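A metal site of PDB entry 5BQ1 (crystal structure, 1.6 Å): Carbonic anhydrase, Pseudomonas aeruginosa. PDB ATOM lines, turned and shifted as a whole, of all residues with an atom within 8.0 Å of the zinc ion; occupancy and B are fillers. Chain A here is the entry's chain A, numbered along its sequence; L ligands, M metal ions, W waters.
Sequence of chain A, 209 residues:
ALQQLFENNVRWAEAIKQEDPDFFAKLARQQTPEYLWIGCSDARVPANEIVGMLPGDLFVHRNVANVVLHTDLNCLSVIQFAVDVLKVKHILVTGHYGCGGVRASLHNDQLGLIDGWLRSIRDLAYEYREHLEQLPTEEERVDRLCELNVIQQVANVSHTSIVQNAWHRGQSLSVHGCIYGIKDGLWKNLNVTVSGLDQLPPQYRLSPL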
ATOM      1  N   GLY A  39      -7.405  -2.670   4.904  1.00  0.00           N
ATOM      2  CA  GLY A  39      -7.182  -2.594   6.339  1.00  0.00           C
ATOM      3  C   GLY A  39      -8.165  -3.437   7.107  1.00  0.00           C
ATOM      4  O   GLY A  39      -8.938  -4.193   6.532  1.00  0.00           O
ATOM      5  N   CYS A  40      -8.093  -3.338   8.433  1.00  0.00           N
ATOM      6  CA  CYS A  40      -8.965  -4.136   9.293  1.00  0.00           C
ATOM      7  C   CYS A  40     -10.329  -3.494   9.412  1.00  0.00           C
ATOM      8  O   CYS A  40     -10.468  -2.271   9.370  1.00  0.00           O
ATOM      9  CB  CYS A  40      -8.333  -4.302  10.677  1.00  0.00           C
ATOM     10  SG  CYS A  40      -9.205  -5.465  11.777  1.00  0.00           S
ATOM     11  N   SER A  41     -11.346  -4.336   9.568  1.00  0.00           N
ATOM     12  CA  SER A  41     -12.708  -3.888   9.859  1.00  0.00           C
ATOM     13  C   SER A  41     -12.861  -3.135  11.178  1.00  0.00           C
ATOM     14  O   SER A  41     -13.853  -2.434  11.352  1.00  0.00           O
ATOM     15  CB  SER A  41     -13.653  -5.087   9.856  1.00  0.00           C
ATOM     16  OG  SER A  41     -13.696  -5.655   8.543  1.00  0.00           O
ATOM     17  N   ASP A  42     -11.910  -3.313  12.098  1.00  0.00           N
ATOM     18  CA  ASP A  42     -11.896  -2.677  13.423  1.00  0.00           C
ATOM     19  C   ASP A  42     -12.415  -1.245  13.343  1.00  0.00           C
ATOM     20  O   ASP A  42     -11.907  -0.429  12.579  1.00  0.00           O
ATOM     21  CB  ASP A  42     -10.467  -2.701  13.988  1.00  0.00           C
ATOM     22  CG  ASP A  42     -10.399  -2.308  15.445  1.00  0.00           C
ATOM     23  OD1 ASP A  42     -10.934  -1.238  15.825  1.00  0.00           O
ATOM     24  OD2 ASP A  42      -9.803  -3.082  16.216  1.00  0.00           O
ATOM     25  N   ALA A  43     -13.427  -0.963  14.148  1.00  0.00           N
ATOM     26  CA  ALA A  43     -14.122   0.312  14.092  1.00  0.00           C
ATOM     27  C   ALA A  43     -13.190   1.479  14.383  1.00  0.00           C
ATOM     28  O   ALA A  43     -13.468   2.618  14.020  1.00  0.00           O
ATOM     29  CB  ALA A  43     -15.301   0.316  15.064  1.00  0.00           C
ATOM     30  N   ARG A  44     -12.088   1.194  15.058  1.00  0.00           N
ATOM     31  CA  ARG A  44     -11.158   2.229  15.462  1.00  0.00           C
ATOM     32  C   ARG A  44     -10.174   2.626  14.354  1.00  0.00           C
ATOM     33  O   ARG A  44      -9.347   3.526  14.558  1.00  0.00           O
ATOM     34  CB  ARG A  44     -10.397   1.785  16.702  1.00  0.00           C
ATOM     35  CG  ARG A  44     -11.332   1.575  17.881  1.00  0.00           C
ATOM     36  CD  ARG A  44     -10.710   0.775  19.015  1.00  0.00           C
ATOM     37  NE  ARG A  44     -10.337  -0.573  18.612  1.00  0.00           N
ATOM     38  CZ  ARG A  44      -9.864  -1.495  19.442  1.00  0.00           C
ATOM     39  NH1 ARG A  44      -9.729  -1.207  20.743  1.00  0.00           N
ATOM     40  NH2 ARG A  44      -9.545  -2.703  18.996  1.00  0.00           N
ATOM     41  N   VAL A  45     -10.269   1.989  13.188  1.00  0.00           N
ATOM     42  CA  VAL A  45      -9.307   2.273  12.135  1.00  0.00           C
ATOM     43  C   VAL A  45      -9.963   2.685  10.802  1.00  0.00           C
ATOM     44  O   VAL A  45      -9.750   2.052   9.762  1.00  0.00           O
ATOM     45  CB  VAL A  45      -8.385   1.033  11.933  1.00  0.00           C
ATOM     46  CG1 VAL A  45      -7.125   1.393  11.138  1.00  0.00           C
ATOM     47  CG2 VAL A  45      -7.970   0.453  13.317  1.00  0.00           C
ATOM     48  N   ASN A  63     -11.421  -5.947   6.121  1.00  0.00           N
ATOM     49  CA  ASN A  63     -11.826  -7.298   6.500  1.00  0.00           C
ATOM     50  C   ASN A  63     -11.199  -7.631   7.848  1.00  0.00           C
ATOM     51  O   ASN A  63     -10.457  -6.818   8.406  1.00  0.00           O
ATOM     52  CB  ASN A  63     -11.447  -8.326   5.416  1.00  0.00           C
ATOM     53  CG  ASN A  63      -9.947  -8.534   5.261  1.00  0.00           C
ATOM     54  OD1 ASN A  63      -9.218  -8.671   6.242  1.00  0.00           O
ATOM     55  ND2 ASN A  63      -9.482  -8.652   4.009  1.00  0.00           N
ATOM     56  N   VAL A  64     -11.513  -8.801   8.413  1.00  0.00           N
ATOM     57  CA  VAL A  64     -10.970  -9.125   9.731  1.00  0.00           C
ATOM     58  C   VAL A  64      -9.463  -9.363   9.636  1.00  0.00           C
ATOM     59  O   VAL A  64      -9.019 -10.294   8.961  1.00  0.00           O
ATOM     60  CB  VAL A  64     -11.667 -10.354  10.303  1.00  0.00           C
ATOM     61  CG1 VAL A  64     -10.981 -10.826  11.595  1.00  0.00           C
ATOM     62  CG2 VAL A  64     -13.126 -10.041  10.555  1.00  0.00           C
ATOM     63  N   ALA A  65      -8.704  -8.502  10.308  1.00  0.00           N
ATOM     64  CA  ALA A  65      -7.239  -8.545  10.386  1.00  0.00           C
ATOM     65  C   ALA A  65      -6.503  -8.280   9.066  1.00  0.00           C
ATOM     66  O   ALA A  65      -5.328  -8.616   8.941  1.00  0.00           O
ATOM     67  CB  ALA A  65      -6.773  -9.879  10.996  1.00  0.00           C
ATOM     68  N   ASN A  66      -7.171  -7.622   8.104  1.00  0.00           N
ATOM     69  CA  ASN A  66      -6.534  -7.091   6.901  1.00  0.00           C
ATOM     70  C   ASN A  66      -5.635  -8.117   6.209  1.00  0.00           C
ATOM     71  O   ASN A  66      -4.467  -7.829   5.883  1.00  0.00           O
ATOM     72  CB  ASN A  66      -5.740  -5.763   7.179  1.00  0.00           C
ATOM     73  CG  ASN A  66      -4.783  -5.842   8.372  1.00  0.00           C
ATOM     74  OD1 ASN A  66      -5.143  -5.481   9.499  1.00  0.00           O
ATOM     75  ND2 ASN A  66      -3.558  -6.261   8.115  1.00  0.00           N
ATOM     76  N   THR A  94      -2.715  -1.583   5.460  1.00  0.00           N
ATOM     77  CA  THR A  94      -2.568  -1.008   6.783  1.00  0.00           C
ATOM     78  C   THR A  94      -3.098  -1.969   7.829  1.00  0.00           C
ATOM     79  O   THR A  94      -4.297  -2.237   7.867  1.00  0.00           O
ATOM     80  CB  THR A  94      -3.315   0.339   6.922  1.00  0.00           C
ATOM     81  OG1 THR A  94      -2.756   1.292   5.999  1.00  0.00           O
ATOM     82  CG2 THR A  94      -3.188   0.880   8.350  1.00  0.00           C
ATOM     83  N   GLY A  95      -2.209  -2.490   8.666  1.00  0.00           N
ATOM     84  CA  GLY A  95      -2.633  -3.248   9.833  1.00  0.00           C
ATOM     85  C   GLY A  95      -2.652  -2.303  11.022  1.00  0.00           C
ATOM     86  O   GLY A  95      -2.445  -1.105  10.874  1.00  0.00           O
ATOM     87  N   HIS A  96      -2.927  -2.833  12.201  1.00  0.00           N
ATOM     88  CA  HIS A  96      -2.908  -1.978  13.375  1.00  0.00           C
ATOM     89  C   HIS A  96      -2.506  -2.763  14.617  1.00  0.00           C
ATOM     90  O   HIS A  96      -2.752  -3.979  14.720  1.00  0.00           O
ATOM     91  CB  HIS A  96      -4.262  -1.297  13.567  1.00  0.00           C
ATOM     92  CG  HIS A  96      -5.354  -2.227  13.990  1.00  0.00           C
ATOM     93  ND1 HIS A  96      -5.740  -2.378  15.296  1.00  0.00           N
ATOM     94  CD2 HIS A  96      -6.136  -3.072  13.269  1.00  0.00           C
ATOM     95  CE1 HIS A  96      -6.712  -3.277  15.372  1.00  0.00           C
ATOM     96  NE2 HIS A  96      -6.959  -3.711  14.158  1.00  0.00           N
ATOM     97  N   TYR A  97      -1.860  -2.083  15.544  1.00  0.00           N
ATOM     98  CA  TYR A  97      -1.495  -2.721  16.786  1.00  0.00           C
ATOM     99  C   TYR A  97      -2.762  -3.039  17.581  1.00  0.00           C
ATOM    100  O   TYR A  97      -3.790  -2.379  17.400  1.00  0.00           O
ATOM    101  CB  TYR A  97      -0.562  -1.824  17.608  1.00  0.00           C
ATOM    102  CG  TYR A  97       0.790  -1.607  16.960  1.00  0.00           C
ATOM    103  CD1 TYR A  97       1.654  -2.672  16.736  1.00  0.00           C
ATOM    104  CD2 TYR A  97       1.213  -0.334  16.596  1.00  0.00           C
ATOM    105  CE1 TYR A  97       2.905  -2.477  16.153  1.00  0.00           C
ATOM    106  CE2 TYR A  97       2.451  -0.122  16.025  1.00  0.00           C
ATOM    107  CZ  TYR A  97       3.298  -1.192  15.816  1.00  0.00           C
ATOM    108  OH  TYR A  97       4.526  -0.979  15.241  1.00  0.00           O
ATOM    109  N   GLY A  98      -2.688  -4.063  18.419  1.00  0.00           N
ATOM    110  CA  GLY A  98      -3.815  -4.444  19.250  1.00  0.00           C
ATOM    111  C   GLY A  98      -4.961  -5.065  18.480  1.00  0.00           C
ATOM    112  O   GLY A  98      -6.093  -5.099  18.961  1.00  0.00           O
ATOM    113  N   CYS A  99      -4.668  -5.574  17.288  1.00  0.00           N
ATOM    114  CA  CYS A  99      -5.691  -6.181  16.448  1.00  0.00           C
ATOM    115  C   CYS A  99      -6.207  -7.474  17.061  1.00  0.00           C
ATOM    116  O   CYS A  99      -5.425  -8.390  17.339  1.00  0.00           O
ATOM    117  CB  CYS A  99      -5.140  -6.446  15.035  1.00  0.00           C
ATOM    118  SG  CYS A  99      -6.320  -7.165  13.857  1.00  0.00           S
ATOM    119  N   GLY A 100      -7.524  -7.559  17.213  1.00  0.00           N
ATOM    120  CA  GLY A 100      -8.142  -8.714  17.854  1.00  0.00           C
ATOM    121  C   GLY A 100      -8.020  -9.994  17.046  1.00  0.00           C
ATOM    122  O   GLY A 100      -7.884 -11.083  17.605  1.00  0.00           O
ATOM    123  N   GLY A 101      -8.057  -9.863  15.721  1.00  0.00           N
ATOM    124  CA  GLY A 101      -7.923 -11.019  14.858  1.00  0.00           C
ATOM    125  C   GLY A 101      -6.529 -11.617  14.992  1.00  0.00           C
ATOM    126  O   GLY A 101      -6.347 -12.840  15.063  1.00  0.00           O
ATOM    127  N   VAL A 102      -5.533 -10.733  15.022  1.00  0.00           N
ATOM    128  CA  VAL A 102      -4.150 -11.150  15.213  1.00  0.00           C
ATOM    129  C   VAL A 102      -3.988 -11.776  16.603  1.00  0.00           C
ATOM    130  O   VAL A 102      -3.388 -12.858  16.742  1.00  0.00           O
ATOM    131  CB  VAL A 102      -3.187  -9.968  15.013  1.00  0.00           C
ATOM    132  CG1 VAL A 102      -1.759 -10.388  15.312  1.00  0.00           C
ATOM    133  CG2 VAL A 102      -3.300  -9.441  13.576  1.00  0.00           C
ATOM    134  N   ARG A 103      -4.533 -11.117  17.620  1.00  0.00           N
ATOM    135  CA  ARG A 103      -4.446 -11.630  18.985  1.00  0.00           C
ATOM    136  C   ARG A 103      -5.029 -13.044  19.101  1.00  0.00           C
ATOM    137  O   ARG A 103      -4.429 -13.915  19.717  1.00  0.00           O
ATOM    138  CB  ARG A 103      -5.161 -10.669  19.944  1.00  0.00           C
ATOM    139  CG  ARG A 103      -5.310 -11.232  21.355  1.00  0.00           C
ATOM    140  CD  ARG A 103      -5.682 -10.152  22.379  1.00  0.00           C
ATOM    141  NE  ARG A 103      -4.526  -9.370  22.789  1.00  0.00           N
ATOM    142  CZ  ARG A 103      -4.344  -8.083  22.503  1.00  0.00           C
ATOM    143  NH1 ARG A 103      -5.261  -7.413  21.817  1.00  0.00           N
ATOM    144  NH2 ARG A 103      -3.242  -7.473  22.924  1.00  0.00           N
ATOM    145  N   CYS A 146       1.283  -8.375  14.477  1.00  0.00           N
ATOM    146  CA  CYS A 146       0.531  -7.399  13.666  1.00  0.00           C
ATOM    147  C   CYS A 146       1.402  -6.837  12.534  1.00  0.00           C
ATOM    148  O   CYS A 146       0.932  -6.670  11.408  1.00  0.00           O
ATOM    149  CB  CYS A 146      -0.003  -6.258  14.533  1.00  0.00           C
ATOM    150  SG  CYS A 146      -1.375  -6.710  15.635  1.00  0.00           S
ATOM    151  N   ASN A 149       2.254  -9.635   9.999  1.00  0.00           N
ATOM    152  CA  ASN A 149       1.073  -9.870   9.175  1.00  0.00           C
ATOM    153  C   ASN A 149       0.994  -8.868   8.023  1.00  0.00           C
ATOM    154  O   ASN A 149       0.761  -9.260   6.873  1.00  0.00           O
ATOM    155  CB  ASN A 149      -0.195  -9.817  10.026  1.00  0.00           C
ATOM    156  CG  ASN A 149      -1.441 -10.214   9.246  1.00  0.00           C
ATOM    157  OD1 ASN A 149      -1.449 -11.218   8.523  1.00  0.00           O
ATOM    158  ND2 ASN A 149      -2.481  -9.386   9.353  1.00  0.00           N
ATOM    159  N   ILE A 182      -3.654   2.164  17.519  1.00  0.00           N
ATOM    160  CA  ILE A 182      -4.930   2.573  18.091  1.00  0.00           C
ATOM    161  C   ILE A 182      -4.725   3.353  19.404  1.00  0.00           C
ATOM    162  O   ILE A 182      -5.580   4.144  19.788  1.00  0.00           O
ATOM    163  CB  ILE A 182      -5.889   1.387  18.336  1.00  0.00           C
ATOM    164  CG1 ILE A 182      -5.196   0.262  19.118  1.00  0.00           C
ATOM    165  CG2 ILE A 182      -6.412   0.873  17.005  1.00  0.00           C
ATOM    166  CD1 ILE A 182      -6.146  -0.855  19.536  1.00  0.00           C
HETATM  167  C1  LIG L   1     -10.942  -7.382  14.433  1.00  0.00           C
HETATM  168  O1  LIG L   1     -10.264  -8.241  13.899  1.00  0.00           O
HETATM  169  O2  LIG L   1     -11.576  -6.492  14.972  1.00  0.00           O
HETATM  170 ZN    ZN M   1      -7.925  -5.503  13.655  1.00  0.00          ZN
HETATM  171  O   HOH W   1      -9.078  -5.477  15.356  1.00  0.00           O
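The zinc ion is bound by water W1 (2.1 Å), NE2 of His 96 (2.1 Å), SG of Cys 40 (2.3 Å) and SG of Cys 99 (2.3 Å). The zinc ion has four donor atoms within binding distance.
Water W1 lies within hydrogen-bond range of the side-chain carboxylate of Asp 42 (2.6 Å), an oxygen (O2) of the ligand (2.7 Å) and the backbone NH of Gly 100 (3.2 Å).
Merely in contact with the zinc ion: Asp 42 (3.8 Å). Along chain A the residues within 4 Å of the zinc ion span positions 40 to 99.
N of Gly 101 is in hydrogen-bond range of O1 of the ligand (3.3 Å). SG of Cys 40 sits close to O1 of the ligand (3.7 Å).
OD2 of Asp 42 is in salt-bridge range of NH2 of Arg 44. The side-chain sulfur (SG) of Cys 40 sits close to the backbone NH (N) of Asp 42. The backbone carbonyl oxygen (O) of His 96 is in hydrogen-bond range of the side-chain sulfur (SG) of Cys 146 (3.2 Å). SG of Cys 40 sits close to N of Ala 65. The side-chain sulfur of Cys 99 lies close to the backbone NH of Gly 101 (3.7 Å).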
